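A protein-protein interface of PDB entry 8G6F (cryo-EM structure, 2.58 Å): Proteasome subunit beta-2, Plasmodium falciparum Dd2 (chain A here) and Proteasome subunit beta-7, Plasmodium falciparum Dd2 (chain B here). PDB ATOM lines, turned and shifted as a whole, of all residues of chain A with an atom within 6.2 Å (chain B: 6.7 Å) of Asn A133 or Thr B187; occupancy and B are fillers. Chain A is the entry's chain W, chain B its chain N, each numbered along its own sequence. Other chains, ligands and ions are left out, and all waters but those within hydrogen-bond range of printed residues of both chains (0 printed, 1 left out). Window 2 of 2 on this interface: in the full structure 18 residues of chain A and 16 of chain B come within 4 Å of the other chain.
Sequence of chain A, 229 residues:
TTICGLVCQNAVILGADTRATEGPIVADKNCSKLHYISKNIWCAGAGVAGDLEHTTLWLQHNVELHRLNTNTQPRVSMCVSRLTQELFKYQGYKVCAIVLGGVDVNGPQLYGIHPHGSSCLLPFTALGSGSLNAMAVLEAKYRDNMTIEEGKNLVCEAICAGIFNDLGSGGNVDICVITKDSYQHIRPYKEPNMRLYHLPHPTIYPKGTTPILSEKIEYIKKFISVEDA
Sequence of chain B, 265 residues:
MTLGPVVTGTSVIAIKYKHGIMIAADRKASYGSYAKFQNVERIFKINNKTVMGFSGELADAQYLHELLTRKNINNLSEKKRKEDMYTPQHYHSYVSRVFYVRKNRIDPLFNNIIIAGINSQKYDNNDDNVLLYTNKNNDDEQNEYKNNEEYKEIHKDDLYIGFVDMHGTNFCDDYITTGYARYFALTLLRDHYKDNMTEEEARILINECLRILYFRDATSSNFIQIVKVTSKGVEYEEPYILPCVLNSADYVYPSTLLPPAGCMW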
ATOM      1  N   THR A   2      34.755 -28.646 -19.119  1.00  0.00           N
ATOM      2  CA  THR A   2      33.852 -29.131 -20.153  1.00  0.00           C
ATOM      3  C   THR A   2      34.684 -29.307 -21.410  1.00  0.00           C
ATOM      4  O   THR A   2      35.146 -28.319 -21.992  1.00  0.00           O
ATOM      5  CB  THR A   2      32.694 -28.167 -20.400  1.00  0.00           C
ATOM      6  OG1 THR A   2      32.215 -27.657 -19.152  1.00  0.00           O
ATOM      7  CG2 THR A   2      31.562 -28.869 -21.119  1.00  0.00           C
ATOM      8  N   SER A 129      33.359 -32.046 -15.634  1.00  0.00           N
ATOM      9  CA  SER A 129      32.259 -31.813 -14.705  1.00  0.00           C
ATOM     10  C   SER A 129      31.042 -31.225 -15.408  1.00  0.00           C
ATOM     11  O   SER A 129      29.914 -31.419 -14.947  1.00  0.00           O
ATOM     12  CB  SER A 129      32.717 -30.900 -13.571  1.00  0.00           C
ATOM     13  OG  SER A 129      33.471 -29.810 -14.062  1.00  0.00           O
ATOM     14  N   GLY A 130      31.243 -30.511 -16.514  1.00  0.00           N
ATOM     15  CA  GLY A 130      30.170 -30.000 -17.339  1.00  0.00           C
ATOM     16  C   GLY A 130      29.714 -30.964 -18.407  1.00  0.00           C
ATOM     17  O   GLY A 130      28.941 -30.586 -19.297  1.00  0.00           O
ATOM     18  N   SER A 131      30.178 -32.213 -18.335  1.00  0.00           N
ATOM     19  CA  SER A 131      29.896 -33.180 -19.383  1.00  0.00           C
ATOM     20  C   SER A 131      28.405 -33.426 -19.543  1.00  0.00           C
ATOM     21  O   SER A 131      27.946 -33.669 -20.656  1.00  0.00           O
ATOM     22  CB  SER A 131      30.611 -34.496 -19.089  1.00  0.00           C
ATOM     23  OG  SER A 131      30.117 -35.099 -17.912  1.00  0.00           O
ATOM     24  N   LEU A 132      27.630 -33.366 -18.460  1.00  0.00           N
ATOM     25  CA  LEU A 132      26.204 -33.662 -18.575  1.00  0.00           C
ATOM     26  C   LEU A 132      25.460 -32.553 -19.312  1.00  0.00           C
ATOM     27  O   LEU A 132      24.590 -32.833 -20.142  1.00  0.00           O
ATOM     28  CB  LEU A 132      25.604 -33.895 -17.189  1.00  0.00           C
ATOM     29  CG  LEU A 132      26.123 -35.112 -16.409  1.00  0.00           C
ATOM     30  CD1 LEU A 132      25.108 -35.564 -15.383  1.00  0.00           C
ATOM     31  CD2 LEU A 132      26.479 -36.267 -17.317  1.00  0.00           C
ATOM     32  N   ASN A 133      25.799 -31.292 -19.048  1.00  0.00           N
ATOM     33  CA  ASN A 133      25.196 -30.196 -19.802  1.00  0.00           C
ATOM     34  C   ASN A 133      25.628 -30.230 -21.265  1.00  0.00           C
ATOM     35  O   ASN A 133      24.798 -30.076 -22.179  1.00  0.00           O
ATOM     36  CB  ASN A 133      25.568 -28.862 -19.159  1.00  0.00           C
ATOM     37  CG  ASN A 133      25.409 -28.874 -17.649  1.00  0.00           C
ATOM     38  OD1 ASN A 133      26.388 -28.875 -16.907  1.00  0.00           O
ATOM     39  ND2 ASN A 133      24.168 -28.882 -17.188  1.00  0.00           N
ATOM     40  N   ALA A 134      26.922 -30.449 -21.510  1.00  0.00           N
ATOM     41  CA  ALA A 134      27.386 -30.546 -22.889  1.00  0.00           C
ATOM     42  C   ALA A 134      26.700 -31.696 -23.612  1.00  0.00           C
ATOM     43  O   ALA A 134      26.323 -31.570 -24.782  1.00  0.00           O
ATOM     44  CB  ALA A 134      28.903 -30.714 -22.919  1.00  0.00           C
ATOM     45  N   MET A 135      26.525 -32.827 -22.928  1.00  0.00           N
ATOM     46  CA  MET A 135      25.885 -33.984 -23.529  1.00  0.00           C
ATOM     47  C   MET A 135      24.412 -33.736 -23.781  1.00  0.00           C
ATOM     48  O   MET A 135      23.863 -34.254 -24.753  1.00  0.00           O
ATOM     49  CB  MET A 135      26.062 -35.205 -22.631  1.00  0.00           C
ATOM     50  CG  MET A 135      25.924 -36.522 -23.360  1.00  0.00           C
ATOM     51  SD  MET A 135      27.440 -36.990 -24.211  1.00  0.00           S
ATOM     52  CE  MET A 135      28.326 -37.782 -22.876  1.00  0.00           C
ATOM     53  N   ALA A 136      23.749 -32.975 -22.917  1.00  0.00           N
ATOM     54  CA  ALA A 136      22.375 -32.584 -23.202  1.00  0.00           C
ATOM     55  C   ALA A 136      22.302 -31.828 -24.519  1.00  0.00           C
ATOM     56  O   ALA A 136      21.480 -32.143 -25.389  1.00  0.00           O
ATOM     57  CB  ALA A 136      21.831 -31.733 -22.061  1.00  0.00           C
ATOM     58  N   VAL A 137      23.182 -30.843 -24.697  1.00  0.00           N
ATOM     59  CA  VAL A 137      23.176 -30.078 -25.944  1.00  0.00           C
ATOM     60  C   VAL A 137      23.448 -30.994 -27.135  1.00  0.00           C
ATOM     61  O   VAL A 137      22.753 -30.942 -28.160  1.00  0.00           O
ATOM     62  CB  VAL A 137      24.196 -28.929 -25.877  1.00  0.00           C
ATOM     63  CG1 VAL A 137      24.290 -28.229 -27.219  1.00  0.00           C
ATOM     64  CG2 VAL A 137      23.811 -27.950 -24.798  1.00  0.00           C
ATOM     65  N   LEU A 138      24.469 -31.845 -27.015  1.00  0.00           N
ATOM     66  CA  LEU A 138      24.858 -32.702 -28.131  1.00  0.00           C
ATOM     67  C   LEU A 138      23.760 -33.696 -28.483  1.00  0.00           C
ATOM     68  O   LEU A 138      23.473 -33.920 -29.662  1.00  0.00           O
ATOM     69  CB  LEU A 138      26.151 -33.439 -27.795  1.00  0.00           C
ATOM     70  CG  LEU A 138      27.407 -32.576 -27.695  1.00  0.00           C
ATOM     71  CD1 LEU A 138      28.525 -33.344 -27.016  1.00  0.00           C
ATOM     72  CD2 LEU A 138      27.837 -32.102 -29.066  1.00  0.00           C
ATOM     73  N   ALA A 158      27.613 -26.504 -26.889  1.00  0.00           N
ATOM     74  CA  ALA A 158      27.823 -27.482 -25.827  1.00  0.00           C
ATOM     75  C   ALA A 158      28.790 -26.953 -24.773  1.00  0.00           C
ATOM     76  O   ALA A 158      28.549 -27.080 -23.563  1.00  0.00           O
ATOM     77  CB  ALA A 158      28.339 -28.789 -26.425  1.00  0.00           C
ATOM     78  N   ALA A 161      27.097 -24.282 -22.714  1.00  0.00           N
ATOM     79  CA  ALA A 161      26.205 -24.897 -21.741  1.00  0.00           C
ATOM     80  C   ALA A 161      26.984 -25.371 -20.526  1.00  0.00           C
ATOM     81  O   ALA A 161      26.607 -25.094 -19.381  1.00  0.00           O
ATOM     82  CB  ALA A 161      25.454 -26.060 -22.386  1.00  0.00           C
ATOM     83  N   GLY A 162      28.085 -26.085 -20.761  1.00  0.00           N
ATOM     84  CA  GLY A 162      28.916 -26.514 -19.648  1.00  0.00           C
ATOM     85  C   GLY A 162      29.437 -25.347 -18.832  1.00  0.00           C
ATOM     86  O   GLY A 162      29.378 -25.355 -17.601  1.00  0.00           O
ATOM     87  N   ASN A 165      26.525 -23.668 -16.782  1.00  0.00           N
ATOM     88  CA  ASN A 165      25.762 -24.489 -15.855  1.00  0.00           C
ATOM     89  C   ASN A 165      26.615 -25.241 -14.845  1.00  0.00           C
ATOM     90  O   ASN A 165      26.068 -25.730 -13.852  1.00  0.00           O
ATOM     91  CB  ASN A 165      24.907 -25.498 -16.629  1.00  0.00           C
ATOM     92  CG  ASN A 165      23.937 -24.830 -17.576  1.00  0.00           C
ATOM     93  OD1 ASN A 165      23.894 -25.146 -18.761  1.00  0.00           O
ATOM     94  ND2 ASN A 165      23.149 -23.905 -17.057  1.00  0.00           N
ATOM     95  N   ASP A 166      27.924 -25.343 -15.059  1.00  0.00           N
ATOM     96  CA  ASP A 166      28.817 -26.051 -14.152  1.00  0.00           C
ATOM     97  C   ASP A 166      29.747 -25.052 -13.479  1.00  0.00           C
ATOM     98  O   ASP A 166      30.303 -24.172 -14.143  1.00  0.00           O
ATOM     99  CB  ASP A 166      29.616 -27.112 -14.906  1.00  0.00           C
ATOM    100  CG  ASP A 166      30.750 -27.684 -14.089  1.00  0.00           C
ATOM    101  OD1 ASP A 166      30.571 -27.878 -12.873  1.00  0.00           O
ATOM    102  OD2 ASP A 166      31.823 -27.944 -14.665  1.00  0.00           O
ATOM    103  N   ALA B 181      17.239 -34.843 -14.224  1.00  0.00           N
ATOM    104  CA  ALA B 181      16.766 -33.756 -15.067  1.00  0.00           C
ATOM    105  C   ALA B 181      17.541 -32.480 -14.803  1.00  0.00           C
ATOM    106  O   ALA B 181      17.780 -31.708 -15.734  1.00  0.00           O
ATOM    107  CB  ALA B 181      15.273 -33.524 -14.847  1.00  0.00           C
ATOM    108  N   ARG B 182      17.985 -32.273 -13.561  1.00  0.00           N
ATOM    109  CA  ARG B 182      18.668 -31.042 -13.193  1.00  0.00           C
ATOM    110  C   ARG B 182      19.886 -30.767 -14.056  1.00  0.00           C
ATOM    111  O   ARG B 182      20.389 -29.640 -14.051  1.00  0.00           O
ATOM    112  CB  ARG B 182      19.082 -31.097 -11.725  1.00  0.00           C
ATOM    113  CG  ARG B 182      17.912 -31.009 -10.769  1.00  0.00           C
ATOM    114  CD  ARG B 182      18.325 -30.624  -9.366  1.00  0.00           C
ATOM    115  NE  ARG B 182      19.248 -29.496  -9.342  1.00  0.00           N
ATOM    116  CZ  ARG B 182      20.516 -29.555  -8.953  1.00  0.00           C
ATOM    117  NH1 ARG B 182      21.070 -30.690  -8.555  1.00  0.00           N
ATOM    118  NH2 ARG B 182      21.246 -28.446  -8.961  1.00  0.00           N
ATOM    119  N   TYR B 183      20.392 -31.764 -14.774  1.00  0.00           N
ATOM    120  CA  TYR B 183      21.460 -31.540 -15.738  1.00  0.00           C
ATOM    121  C   TYR B 183      20.918 -31.373 -17.153  1.00  0.00           C
ATOM    122  O   TYR B 183      20.964 -30.273 -17.712  1.00  0.00           O
ATOM    123  CB  TYR B 183      22.456 -32.698 -15.654  1.00  0.00           C
ATOM    124  CG  TYR B 183      23.210 -32.686 -14.353  1.00  0.00           C
ATOM    125  CD1 TYR B 183      22.664 -33.246 -13.210  1.00  0.00           C
ATOM    126  CD2 TYR B 183      24.454 -32.085 -14.257  1.00  0.00           C
ATOM    127  CE1 TYR B 183      23.342 -33.219 -12.013  1.00  0.00           C
ATOM    128  CE2 TYR B 183      25.139 -32.057 -13.068  1.00  0.00           C
ATOM    129  CZ  TYR B 183      24.580 -32.623 -11.947  1.00  0.00           C
ATOM    130  OH  TYR B 183      25.265 -32.595 -10.760  1.00  0.00           O
ATOM    131  N   PHE B 184      20.299 -32.416 -17.697  1.00  0.00           N
ATOM    132  CA  PHE B 184      19.902 -32.395 -19.101  1.00  0.00           C
ATOM    133  C   PHE B 184      18.723 -31.458 -19.329  1.00  0.00           C
ATOM    134  O   PHE B 184      18.799 -30.513 -20.130  1.00  0.00           O
ATOM    135  CB  PHE B 184      19.563 -33.815 -19.559  1.00  0.00           C
ATOM    136  CG  PHE B 184      20.606 -34.835 -19.195  1.00  0.00           C
ATOM    137  CD1 PHE B 184      21.794 -34.910 -19.894  1.00  0.00           C
ATOM    138  CD2 PHE B 184      20.397 -35.720 -18.156  1.00  0.00           C
ATOM    139  CE1 PHE B 184      22.751 -35.845 -19.565  1.00  0.00           C
ATOM    140  CE2 PHE B 184      21.352 -36.658 -17.824  1.00  0.00           C
ATOM    141  CZ  PHE B 184      22.528 -36.717 -18.529  1.00  0.00           C
ATOM    142  N   ALA B 185      17.620 -31.705 -18.627  1.00  0.00           N
ATOM    143  CA  ALA B 185      16.436 -30.895 -18.841  1.00  0.00           C
ATOM    144  C   ALA B 185      16.695 -29.463 -18.422  1.00  0.00           C
ATOM    145  O   ALA B 185      16.178 -28.529 -19.033  1.00  0.00           O
ATOM    146  CB  ALA B 185      15.253 -31.473 -18.067  1.00  0.00           C
ATOM    147  N   LEU B 186      17.491 -29.271 -17.371  1.00  0.00           N
ATOM    148  CA  LEU B 186      17.750 -27.921 -16.896  1.00  0.00           C
ATOM    149  C   LEU B 186      18.604 -27.143 -17.885  1.00  0.00           C
ATOM    150  O   LEU B 186      18.374 -25.950 -18.096  1.00  0.00           O
ATOM    151  CB  LEU B 186      18.413 -27.963 -15.523  1.00  0.00           C
ATOM    152  CG  LEU B 186      18.474 -26.637 -14.757  1.00  0.00           C
ATOM    153  CD1 LEU B 186      17.117 -25.972 -14.680  1.00  0.00           C
ATOM    154  CD2 LEU B 186      19.021 -26.863 -13.366  1.00  0.00           C
ATOM    155  N   THR B 187      19.589 -27.792 -18.508  1.00  0.00           N
ATOM    156  CA  THR B 187      20.342 -27.130 -19.566  1.00  0.00           C
ATOM    157  C   THR B 187      19.425 -26.737 -20.714  1.00  0.00           C
ATOM    158  O   THR B 187      19.450 -25.593 -21.192  1.00  0.00           O
ATOM    159  CB  THR B 187      21.453 -28.055 -20.055  1.00  0.00           C
ATOM    160  OG1 THR B 187      22.217 -28.510 -18.935  1.00  0.00           O
ATOM    161  CG2 THR B 187      22.365 -27.340 -21.022  1.00  0.00           C
ATOM    162  N   LEU B 188      18.582 -27.671 -21.157  1.00  0.00           N
ATOM    163  CA  LEU B 188      17.702 -27.365 -22.278  1.00  0.00           C
ATOM    164  C   LEU B 188      16.711 -26.265 -21.927  1.00  0.00           C
ATOM    165  O   LEU B 188      16.362 -25.451 -22.785  1.00  0.00           O
ATOM    166  CB  LEU B 188      16.967 -28.624 -22.729  1.00  0.00           C
ATOM    167  CG  LEU B 188      17.546 -29.275 -23.981  1.00  0.00           C
ATOM    168  CD1 LEU B 188      19.006 -29.610 -23.774  1.00  0.00           C
ATOM    169  CD2 LEU B 188      16.763 -30.516 -24.346  1.00  0.00           C
ATOM    170  N   LEU B 189      16.254 -26.217 -20.675  1.00  0.00           N
ATOM    171  CA  LEU B 189      15.288 -25.205 -20.267  1.00  0.00           C
ATOM    172  C   LEU B 189      15.946 -23.841 -20.116  1.00  0.00           C
ATOM    173  O   LEU B 189      15.367 -22.821 -20.500  1.00  0.00           O
ATOM    174  CB  LEU B 189      14.628 -25.619 -18.956  1.00  0.00           C
ATOM    175  CG  LEU B 189      13.577 -26.719 -19.063  1.00  0.00           C
ATOM    176  CD1 LEU B 189      13.393 -27.396 -17.726  1.00  0.00           C
ATOM    177  CD2 LEU B 189      12.270 -26.145 -19.557  1.00  0.00           C
ATOM    178  N   ARG B 190      17.148 -23.800 -19.546  1.00  0.00           N
ATOM    179  CA  ARG B 190      17.864 -22.539 -19.436  1.00  0.00           C
ATOM    180  C   ARG B 190      18.229 -21.994 -20.806  1.00  0.00           C
ATOM    181  O   ARG B 190      18.403 -20.782 -20.963  1.00  0.00           O
ATOM    182  CB  ARG B 190      19.114 -22.725 -18.577  1.00  0.00           C
ATOM    183  CG  ARG B 190      18.851 -22.600 -17.089  1.00  0.00           C
ATOM    184  CD  ARG B 190      19.962 -23.208 -16.262  1.00  0.00           C
ATOM    185  NE  ARG B 190      19.705 -23.080 -14.835  1.00  0.00           N
ATOM    186  CZ  ARG B 190      20.481 -23.583 -13.884  1.00  0.00           C
ATOM    187  NH1 ARG B 190      21.574 -24.267 -14.174  1.00  0.00           N
ATOM    188  NH2 ARG B 190      20.147 -23.399 -12.611  1.00  0.00           N
ATOM    189  N   ASP B 191      18.348 -22.865 -21.811  1.00  0.00           N
ATOM    190  CA  ASP B 191      18.579 -22.372 -23.165  1.00  0.00           C
ATOM    191  C   ASP B 191      17.284 -21.917 -23.835  1.00  0.00           C
ATOM    192  O   ASP B 191      17.210 -20.801 -24.356  1.00  0.00           O
ATOM    193  CB  ASP B 191      19.252 -23.450 -24.018  1.00  0.00           C
ATOM    194  CG  ASP B 191      20.752 -23.509 -23.817  1.00  0.00           C
ATOM    195  OD1 ASP B 191      21.339 -22.506 -23.364  1.00  0.00           O
ATOM    196  OD2 ASP B 191      21.347 -24.564 -24.119  1.00  0.00           O
ATOM    197  N   HIS B 192      16.251 -22.761 -23.828  1.00  0.00           N
ATOM    198  CA  HIS B 192      15.141 -22.624 -24.760  1.00  0.00           C
ATOM    199  C   HIS B 192      13.822 -22.211 -24.130  1.00  0.00           C
ATOM    200  O   HIS B 192      12.896 -21.857 -24.867  1.00  0.00           O
ATOM    201  CB  HIS B 192      14.927 -23.945 -25.509  1.00  0.00           C
ATOM    202  CG  HIS B 192      16.168 -24.481 -26.145  1.00  0.00           C
ATOM    203  ND1 HIS B 192      16.892 -23.768 -27.074  1.00  0.00           N
ATOM    204  CD2 HIS B 192      16.813 -25.659 -25.987  1.00  0.00           C
ATOM    205  CE1 HIS B 192      17.934 -24.483 -27.459  1.00  0.00           C
ATOM    206  NE2 HIS B 192      17.908 -25.635 -26.815  1.00  0.00           N
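The side-chain hydroxyl of Thr B187 lies within hydrogen-bond range of the side-chain amide nitrogen of Asn A133, at 2.6 Å.
NH1 of Arg B190 lies close to ND2 of Asn A165, 3.3 Å away.
O of Ala A161 sits close to OD1 of Asn A165 (2.8 Å).
OG1 of Thr B187 is in hydrogen-bond range of O of Tyr B183 (2.5 Å).
Among the printed residues, pairs that only touch across the chains: Leu A132 with Phe B184, Asn A165 with Thr B187, Asn A133 with Tyr B183, Ala A136 with Phe B184, Leu A132 with Tyr B183, Ala A161 with Thr B187 and Ala A136 with Leu B188.
Ser A131 touches none of the printed residues of chain B.
Asn A133 touches just these residues of chain B: Tyr B183 (3.5 Å) and Thr B187 (2.6 Å).
Of the printed residues of chain B, Asn A165 touches Thr B187 (3.5 Å) and Arg B190 (3.3 Å).
Thr B187 touches just these residues of chain A: Asn A133, Ala A161 and Asn A165.
Printed residues of chain A within 4 Å of Leu B188: Ala A136.
The nearest residue of chain B that does not touch Asn A133 is Arg B182 (5.0 Å).
Of the 12 printed residues of chain B, 5 touch a printed residue of chain A.
Printed residues of chain A that touch a printed residue of chain B: Leu A132, Asn A133, Ala A136, Ala A161 and Asn A165.
Hydrophobic or aromatic side chains of chain A that line the printed part of chain B: Leu A132, Ala A136 and Ala A161.
Among the printed residues, 9 pairs touch across the chains.
Among the printed residues, no Asp or Glu carboxylate lies within 4 Å of a Lys or Arg side-chain nitrogen of the other chain.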
